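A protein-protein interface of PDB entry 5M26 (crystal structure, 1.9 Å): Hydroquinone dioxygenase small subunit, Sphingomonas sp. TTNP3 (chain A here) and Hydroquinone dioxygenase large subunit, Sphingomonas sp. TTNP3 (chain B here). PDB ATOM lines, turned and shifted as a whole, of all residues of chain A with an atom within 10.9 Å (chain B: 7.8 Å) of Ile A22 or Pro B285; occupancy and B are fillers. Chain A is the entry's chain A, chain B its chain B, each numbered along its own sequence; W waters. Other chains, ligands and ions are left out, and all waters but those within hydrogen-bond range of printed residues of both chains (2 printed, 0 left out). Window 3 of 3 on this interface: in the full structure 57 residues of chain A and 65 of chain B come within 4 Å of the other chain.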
ATOM      1  N   GLY A  18      -6.864   9.166  -2.531  1.00  0.00           N
ATOM      2  CA  GLY A  18      -6.400  10.089  -3.551  1.00  0.00           C
ATOM      3  C   GLY A  18      -7.484  10.679  -4.385  1.00  0.00           C
ATOM      4  O   GLY A  18      -8.668  10.437  -4.139  1.00  0.00           O
ATOM      5  N   VAL A  19      -7.057  11.465  -5.368  1.00  0.00           N
ATOM      6  CA  VAL A  19      -7.943  12.237  -6.218  1.00  0.00           C
ATOM      7  C   VAL A  19      -8.160  11.460  -7.524  1.00  0.00           C
ATOM      8  O   VAL A  19      -7.178  11.144  -8.211  1.00  0.00           O
ATOM      9  CB  VAL A  19      -7.327  13.613  -6.556  1.00  0.00           C
ATOM     10  CG1 VAL A  19      -8.270  14.414  -7.454  1.00  0.00           C
ATOM     11  CG2 VAL A  19      -7.024  14.392  -5.285  1.00  0.00           C
ATOM     12  N   GLU A  20      -9.429  11.136  -7.825  1.00  0.00           N
ATOM     13  CA  GLU A  20      -9.839  10.588  -9.127  1.00  0.00           C
ATOM     14  C   GLU A  20     -10.273  11.783  -9.986  1.00  0.00           C
ATOM     15  O   GLU A  20     -11.085  12.619  -9.559  1.00  0.00           O
ATOM     16  CB  GLU A  20     -11.000   9.566  -8.991  1.00  0.00           C
ATOM     17  CG  GLU A  20     -11.675   9.161 -10.326  1.00  0.00           C
ATOM     18  CD  GLU A  20     -13.197   8.826 -10.250  1.00  0.00           C
ATOM     19  OE1 GLU A  20     -13.993   9.369 -11.081  1.00  0.00           O
ATOM     20  OE2 GLU A  20     -13.611   8.010  -9.390  1.00  0.00           O
ATOM     21  N   ILE A  21      -9.753  11.870 -11.198  1.00  0.00           N
ATOM     22  CA  ILE A  21     -10.022  13.046 -12.014  1.00  0.00           C
ATOM     23  C   ILE A  21     -11.123  12.809 -13.052  1.00  0.00           C
ATOM     24  O   ILE A  21     -11.115  11.786 -13.754  1.00  0.00           O
ATOM     25  CB  ILE A  21      -8.763  13.543 -12.737  1.00  0.00           C
ATOM     26  CG1 ILE A  21      -7.689  13.983 -11.740  1.00  0.00           C
ATOM     27  CG2 ILE A  21      -9.120  14.655 -13.710  1.00  0.00           C
ATOM     28  CD1 ILE A  21      -8.054  15.191 -10.909  1.00  0.00           C
ATOM     29  N   ILE A  22     -12.047  13.776 -13.135  1.00  0.00           N
ATOM     30  CA  ILE A  22     -12.959  13.886 -14.245  1.00  0.00           C
ATOM     31  C   ILE A  22     -12.457  14.988 -15.198  1.00  0.00           C
ATOM     32  O   ILE A  22     -12.231  14.727 -16.380  1.00  0.00           O
ATOM     33  CB  ILE A  22     -14.405  14.122 -13.767  1.00  0.00           C
ATOM     34  CG1 ILE A  22     -14.840  12.933 -12.879  1.00  0.00           C
ATOM     35  CG2 ILE A  22     -15.333  14.277 -14.960  1.00  0.00           C
ATOM     36  CD1 ILE A  22     -16.053  13.200 -12.013  1.00  0.00           C
ATOM     37  N   ASP A  23     -12.249  16.194 -14.674  1.00  0.00           N
ATOM     38  CA  ASP A  23     -11.722  17.301 -15.454  1.00  0.00           C
ATOM     39  C   ASP A  23     -11.143  18.265 -14.442  1.00  0.00           C
ATOM     40  O   ASP A  23     -11.843  19.146 -13.940  1.00  0.00           O
ATOM     41  CB  ASP A  23     -12.847  17.961 -16.254  1.00  0.00           C
ATOM     42  CG  ASP A  23     -12.342  19.018 -17.256  1.00  0.00           C
ATOM     43  OD1 ASP A  23     -11.118  19.212 -17.406  1.00  0.00           O
ATOM     44  OD2 ASP A  23     -13.196  19.664 -17.897  1.00  0.00           O
ATOM     45  N   ASP A  24      -9.874  18.074 -14.097  1.00  0.00           N
ATOM     46  CA  ASP A  24      -9.287  18.845 -13.004  1.00  0.00           C
ATOM     47  C   ASP A  24      -7.812  18.515 -12.935  1.00  0.00           C
ATOM     48  O   ASP A  24      -7.311  17.728 -13.737  1.00  0.00           O
ATOM     49  CB  ASP A  24      -9.971  18.499 -11.661  1.00  0.00           C
ATOM     50  CG  ASP A  24     -10.105  19.707 -10.729  1.00  0.00           C
ATOM     51  OD1 ASP A  24      -9.142  20.487 -10.615  1.00  0.00           O
ATOM     52  OD2 ASP A  24     -11.181  19.883 -10.086  1.00  0.00           O
ATOM     53  N   ASP A  25      -7.129  19.115 -11.972  1.00  0.00           N
ATOM     54  CA  ASP A  25      -5.698  18.857 -11.753  1.00  0.00           C
ATOM     55  C   ASP A  25      -5.580  18.360 -10.318  1.00  0.00           C
ATOM     56  O   ASP A  25      -6.012  19.062  -9.388  1.00  0.00           O
ATOM     57  CB  ASP A  25      -4.922  20.167 -11.979  1.00  0.00           C
ATOM     58  CG  ASP A  25      -3.414  20.031 -11.767  1.00  0.00           C
ATOM     59  OD1 ASP A  25      -2.945  19.061 -11.111  1.00  0.00           O
ATOM     60  OD2 ASP A  25      -2.695  20.943 -12.242  1.00  0.00           O
ATOM     61  N   PRO A  26      -5.042  17.144 -10.116  1.00  0.00           N
ATOM     62  CA  PRO A  26      -5.048  16.625  -8.735  1.00  0.00           C
ATOM     63  C   PRO A  26      -4.204  17.469  -7.771  1.00  0.00           C
ATOM     64  O   PRO A  26      -4.358  17.345  -6.555  1.00  0.00           O
ATOM     65  CB  PRO A  26      -4.465  15.226  -8.868  1.00  0.00           C
ATOM     66  CG  PRO A  26      -3.817  15.168 -10.187  1.00  0.00           C
ATOM     67  CD  PRO A  26      -4.415  16.208 -11.071  1.00  0.00           C
ATOM     68  N   ASN A  28      -4.526  20.623  -7.391  1.00  0.00           N
ATOM     69  CA  ASN A  28      -5.461  21.583  -6.771  1.00  0.00           C
ATOM     70  C   ASN A  28      -5.925  21.117  -5.384  1.00  0.00           C
ATOM     71  O   ASN A  28      -6.393  21.936  -4.582  1.00  0.00           O
ATOM     72  CB  ASN A  28      -6.698  21.799  -7.626  1.00  0.00           C
ATOM     73  CG  ASN A  28      -6.398  22.475  -8.955  1.00  0.00           C
ATOM     74  OD1 ASN A  28      -7.195  22.387  -9.874  1.00  0.00           O
ATOM     75  ND2 ASN A  28      -5.274  23.153  -9.052  1.00  0.00           N
ATOM     76  N   TYR A  29      -5.820  19.815  -5.115  1.00  0.00           N
ATOM     77  CA  TYR A  29      -6.332  19.234  -3.871  1.00  0.00           C
ATOM     78  C   TYR A  29      -5.273  19.098  -2.797  1.00  0.00           C
ATOM     79  O   TYR A  29      -5.572  18.698  -1.673  1.00  0.00           O
ATOM     80  CB  TYR A  29      -7.092  17.924  -4.146  1.00  0.00           C
ATOM     81  CG  TYR A  29      -8.245  18.263  -5.056  1.00  0.00           C
ATOM     82  CD1 TYR A  29      -8.080  18.236  -6.446  1.00  0.00           C
ATOM     83  CD2 TYR A  29      -9.457  18.733  -4.527  1.00  0.00           C
ATOM     84  CE1 TYR A  29      -9.095  18.640  -7.286  1.00  0.00           C
ATOM     85  CE2 TYR A  29     -10.488  19.115  -5.355  1.00  0.00           C
ATOM     86  CZ  TYR A  29     -10.301  19.062  -6.734  1.00  0.00           C
ATOM     87  OH  TYR A  29     -11.306  19.462  -7.571  1.00  0.00           O
ATOM     88  N   GLN A 166       0.029  14.396  -3.890  1.00  0.00           N
ATOM     89  CA  GLN A 166      -0.320  13.712  -5.111  1.00  0.00           C
ATOM     90  C   GLN A 166      -0.174  14.692  -6.273  1.00  0.00           C
ATOM     91  O   GLN A 166      -0.665  15.813  -6.193  1.00  0.00           O
ATOM     92  CB  GLN A 166      -1.761  13.184  -5.048  1.00  0.00           C
ATOM     93  CG  GLN A 166      -2.128  12.306  -6.253  1.00  0.00           C
ATOM     94  CD  GLN A 166      -3.582  11.847  -6.254  1.00  0.00           C
ATOM     95  OE1 GLN A 166      -4.169  11.569  -7.307  1.00  0.00           O
ATOM     96  NE2 GLN A 166      -4.167  11.779  -5.087  1.00  0.00           N
ATOM     97  N   GLU A 168      -0.190  13.362  -9.850  1.00  0.00           N
ATOM     98  CA  GLU A 168      -0.781  12.745 -11.040  1.00  0.00           C
ATOM     99  C   GLU A 168      -2.038  11.939 -10.664  1.00  0.00           C
ATOM    100  O   GLU A 168      -2.265  11.663  -9.489  1.00  0.00           O
ATOM    101  CB  GLU A 168       0.250  11.813 -11.698  1.00  0.00           C
ATOM    102  CG  GLU A 168       0.606  10.608 -10.821  1.00  0.00           C
ATOM    103  CD  GLU A 168       1.401   9.528 -11.539  1.00  0.00           C
ATOM    104  OE1 GLU A 168       2.384   9.870 -12.228  1.00  0.00           O
ATOM    105  OE2 GLU A 168       1.047   8.330 -11.400  1.00  0.00           O
ATOM    106  N   ALA A 169      -2.836  11.574 -11.672  1.00  0.00           N
ATOM    107  CA  ALA A 169      -3.885  10.534 -11.572  1.00  0.00           C
ATOM    108  C   ALA A 169      -5.061  10.875 -10.686  1.00  0.00           C
ATOM    109  O   ALA A 169      -5.786   9.966 -10.264  1.00  0.00           O
ATOM    110  CB  ALA A 169      -3.295   9.185 -11.167  1.00  0.00           C
ATOM    111  N   ASP B 276     -17.564  14.097  -3.647  1.00  0.00           N
ATOM    112  CA  ASP B 276     -17.994  14.447  -4.989  1.00  0.00           C
ATOM    113  C   ASP B 276     -17.698  15.939  -5.197  1.00  0.00           C
ATOM    114  O   ASP B 276     -18.316  16.809  -4.554  1.00  0.00           O
ATOM    115  CB  ASP B 276     -19.501  14.169  -5.108  1.00  0.00           C
ATOM    116  CG  ASP B 276     -20.046  14.350  -6.526  1.00  0.00           C
ATOM    117  OD1 ASP B 276     -19.416  15.017  -7.368  1.00  0.00           O
ATOM    118  OD2 ASP B 276     -21.149  13.825  -6.813  1.00  0.00           O
ATOM    119  N   VAL B 277     -16.759  16.238  -6.087  1.00  0.00           N
ATOM    120  CA  VAL B 277     -16.345  17.623  -6.312  1.00  0.00           C
ATOM    121  C   VAL B 277     -16.853  18.137  -7.647  1.00  0.00           C
ATOM    122  O   VAL B 277     -16.533  17.567  -8.696  1.00  0.00           O
ATOM    123  CB  VAL B 277     -14.810  17.750  -6.255  1.00  0.00           C
ATOM    124  CG1 VAL B 277     -14.381  19.186  -6.504  1.00  0.00           C
ATOM    125  CG2 VAL B 277     -14.284  17.236  -4.910  1.00  0.00           C
ATOM    126  N   LYS B 278     -17.627  19.221  -7.608  1.00  0.00           N
ATOM    127  CA  LYS B 278     -18.149  19.848  -8.818  1.00  0.00           C
ATOM    128  C   LYS B 278     -17.715  21.282  -8.952  1.00  0.00           C
ATOM    129  O   LYS B 278     -17.309  21.919  -7.973  1.00  0.00           O
ATOM    130  CB  LYS B 278     -19.674  19.813  -8.837  1.00  0.00           C
ATOM    131  CG  LYS B 278     -20.265  18.429  -8.926  1.00  0.00           C
ATOM    132  CD  LYS B 278     -21.751  18.469  -8.630  1.00  0.00           C
ATOM    133  CE  LYS B 278     -22.428  17.201  -9.126  1.00  0.00           C
ATOM    134  NZ  LYS B 278     -22.378  16.119  -8.092  1.00  0.00           N
ATOM    135  N   ASP B 279     -17.845  21.822 -10.149  1.00  0.00           N
ATOM    136  CA  ASP B 279     -17.549  23.239 -10.330  1.00  0.00           C
ATOM    137  C   ASP B 279     -18.482  24.068  -9.466  1.00  0.00           C
ATOM    138  O   ASP B 279     -19.695  23.828  -9.471  1.00  0.00           O
ATOM    139  CB  ASP B 279     -17.755  23.641 -11.773  1.00  0.00           C
ATOM    140  CG  ASP B 279     -17.216  25.020 -12.048  1.00  0.00           C
ATOM    141  OD1 ASP B 279     -15.993  25.200 -11.913  1.00  0.00           O
ATOM    142  OD2 ASP B 279     -18.008  25.919 -12.361  1.00  0.00           O
ATOM    143  N   SER B 282     -20.858  26.180 -12.100  1.00  0.00           N
ATOM    144  CA  SER B 282     -21.722  25.444 -13.036  1.00  0.00           C
ATOM    145  C   SER B 282     -22.366  24.164 -12.476  1.00  0.00           C
ATOM    146  O   SER B 282     -23.415  23.739 -12.972  1.00  0.00           O
ATOM    147  CB  SER B 282     -20.941  25.103 -14.306  1.00  0.00           C
ATOM    148  OG  SER B 282     -19.892  24.207 -13.990  1.00  0.00           O
ATOM    149  N   GLY B 283     -21.753  23.572 -11.455  1.00  0.00           N
ATOM    150  CA  GLY B 283     -22.157  22.247 -10.958  1.00  0.00           C
ATOM    151  C   GLY B 283     -21.629  21.043 -11.765  1.00  0.00           C
ATOM    152  O   GLY B 283     -21.973  19.893 -11.470  1.00  0.00           O
ATOM    153  N   LYS B 284     -20.791  21.291 -12.771  1.00  0.00           N
ATOM    154  CA  LYS B 284     -20.165  20.188 -13.534  1.00  0.00           C
ATOM    155  C   LYS B 284     -19.205  19.346 -12.692  1.00  0.00           C
ATOM    156  O   LYS B 284     -18.276  19.887 -12.079  1.00  0.00           O
ATOM    157  CB  LYS B 284     -19.409  20.741 -14.735  1.00  0.00           C
ATOM    158  CG  LYS B 284     -20.322  21.339 -15.766  1.00  0.00           C
ATOM    159  CD  LYS B 284     -19.564  21.815 -16.993  1.00  0.00           C
ATOM    160  CE  LYS B 284     -20.568  22.393 -17.975  1.00  0.00           C
ATOM    161  NZ  LYS B 284     -19.975  22.671 -19.315  1.00  0.00           N
ATOM    162  N   PRO B 285     -19.402  18.013 -12.678  1.00  0.00           N
ATOM    163  CA  PRO B 285     -18.428  17.107 -12.059  1.00  0.00           C
ATOM    164  C   PRO B 285     -16.986  17.446 -12.466  1.00  0.00           C
ATOM    165  O   PRO B 285     -16.733  17.755 -13.644  1.00  0.00           O
ATOM    166  CB  PRO B 285     -18.829  15.745 -12.620  1.00  0.00           C
ATOM    167  CG  PRO B 285     -20.312  15.854 -12.805  1.00  0.00           C
ATOM    168  CD  PRO B 285     -20.571  17.281 -13.214  1.00  0.00           C
ATOM    169  N   ARG B 286     -16.071  17.427 -11.489  1.00  0.00           N
ATOM    170  CA  ARG B 286     -14.661  17.722 -11.732  1.00  0.00           C
ATOM    171  C   ARG B 286     -13.736  16.645 -11.184  1.00  0.00           C
ATOM    172  O   ARG B 286     -12.748  16.276 -11.838  1.00  0.00           O
ATOM    173  CB  ARG B 286     -14.272  19.114 -11.200  1.00  0.00           C
ATOM    174  CG  ARG B 286     -14.605  20.254 -12.162  1.00  0.00           C
ATOM    175  CD  ARG B 286     -14.417  21.638 -11.539  1.00  0.00           C
ATOM    176  NE  ARG B 286     -13.041  21.855 -11.080  1.00  0.00           N
ATOM    177  CZ  ARG B 286     -12.496  23.050 -10.832  1.00  0.00           C
ATOM    178  NH1 ARG B 286     -13.184  24.169 -11.027  1.00  0.00           N
ATOM    179  NH2 ARG B 286     -11.240  23.122 -10.404  1.00  0.00           N
ATOM    180  N   ALA B 287     -14.059  16.117 -10.005  1.00  0.00           N
ATOM    181  CA  ALA B 287     -13.200  15.142  -9.342  1.00  0.00           C
ATOM    182  C   ALA B 287     -13.976  14.351  -8.305  1.00  0.00           C
ATOM    183  O   ALA B 287     -15.057  14.742  -7.905  1.00  0.00           O
ATOM    184  CB  ALA B 287     -12.004  15.848  -8.681  1.00  0.00           C
ATOM    185  N   ARG B 288     -13.416  13.235  -7.870  1.00  0.00           N
ATOM    186  CA  ARG B 288     -13.937  12.479  -6.734  1.00  0.00           C
ATOM    187  C   ARG B 288     -12.728  12.220  -5.851  1.00  0.00           C
ATOM    188  O   ARG B 288     -11.728  11.681  -6.325  1.00  0.00           O
ATOM    189  CB  ARG B 288     -14.567  11.166  -7.228  1.00  0.00           C
ATOM    190  CG  ARG B 288     -15.667  11.395  -8.261  1.00  0.00           C
ATOM    191  CD  ARG B 288     -16.500  10.163  -8.594  1.00  0.00           C
ATOM    192  NE  ARG B 288     -17.308   9.687  -7.477  1.00  0.00           N
ATOM    193  CZ  ARG B 288     -17.003   8.647  -6.696  1.00  0.00           C
ATOM    194  NH1 ARG B 288     -15.888   7.952  -6.898  1.00  0.00           N
ATOM    195  NH2 ARG B 288     -17.815   8.304  -5.694  1.00  0.00           N
ATOM    196  N   ARG B 304     -17.514  23.145  -5.460  1.00  0.00           N
ATOM    197  CA  ARG B 304     -18.435  22.730  -4.391  1.00  0.00           C
ATOM    198  C   ARG B 304     -18.260  21.231  -4.165  1.00  0.00           C
ATOM    199  O   ARG B 304     -17.875  20.485  -5.083  1.00  0.00           O
ATOM    200  CB  ARG B 304     -19.896  23.022  -4.761  1.00  0.00           C
ATOM    201  CG  ARG B 304     -20.384  22.153  -5.912  1.00  0.00           C
ATOM    202  CD  ARG B 304     -21.858  22.317  -6.220  1.00  0.00           C
ATOM    203  NE  ARG B 304     -22.038  23.373  -7.165  1.00  0.00           N
ATOM    204  CZ  ARG B 304     -23.144  23.597  -7.863  1.00  0.00           C
ATOM    205  NH1 ARG B 304     -24.210  22.818  -7.732  1.00  0.00           N
ATOM    206  NH2 ARG B 304     -23.162  24.628  -8.708  1.00  0.00           N
HETATM  207  O   HOH W   1      -9.172  24.775  -8.522  1.00  0.00           O
HETATM  208  O   HOH W   2     -11.263   8.897  -5.429  1.00  0.00           O
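Water W2 lies within hydrogen-bond range of O of Arg B288 (3.0 Å) and O of Gly A18 (3.3 Å). Water W1 lies within hydrogen-bond range of NH2 of Arg B286 (3.2 Å) and OD1 of Asn A28 (3.4 Å).
OE2 of Glu A20 lies within salt-bridge range of NH1 of Arg B288 (3.4 Å). N of Ile A22 is in hydrogen-bond range of O of Arg B286 (2.9 Å). O of Arg B286 is in hydrogen-bond range of N of Asp A23 (2.9 Å). The side-chain carboxylate (OD2) of Asp A24 is in salt-bridge range of the guanidinium group (NE) of Arg B286, at 2.9 Å.
The backbone NH of Val A19 lies close to the side-chain amide nitrogen of Gln A166 (2.9 Å). O of Val A19 lies close to O of Ala A169 (2.7 Å). The side-chain hydroxyl of Tyr A29 lies within hydrogen-bond range of the side-chain carboxylate of Asp A24 (2.6 Å). The backbone NH of Arg B286 sits at hydrogen-bond distance from the backbone carbonyl oxygen of Val B277 (2.8 Å). N of Val B277 lies within hydrogen-bond range of O of Ala B287, 2.9 Å away. NH1 of Arg B286 is in salt-bridge range of OD1 of Asp B279 (3.1 Å).
Of the 12 printed residues of chain B, 5 touch a printed residue of chain A. Hydrophobic or aromatic side chains of chain A that line the printed part of chain B: Ile A22 and Tyr A29.
Among the printed residues, pairs that only touch across the chains: Tyr A29 with Val B277, Glu A20 with Ala B287, Val A19 with Arg B288, Ile A22 with Pro B285, Tyr A29 with Ala B287 and Gly A18 with Arg B288.
Ile A22 touches just these residues of chain B: Pro B285 and Arg B286. Of the printed residues of chain B, Asp A23 touches Arg B286. Of the printed residues of chain B, Asp A24 touches Arg B286 (2.9 Å). Asp A25 touches none of the printed residues of chain B. No residue of chain A comes within 4 Å of Lys B278. No residue of chain A comes within 4 Å of Gly B283. Pro B285 touches one residue of chain A. Of the printed residues of chain A, Ala B287 touches Glu A20 (3.3 Å) and Tyr A29 (3.8 Å). The nearest residue of chain A that does not touch Pro B285 is Asp A23 (4.7 Å).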
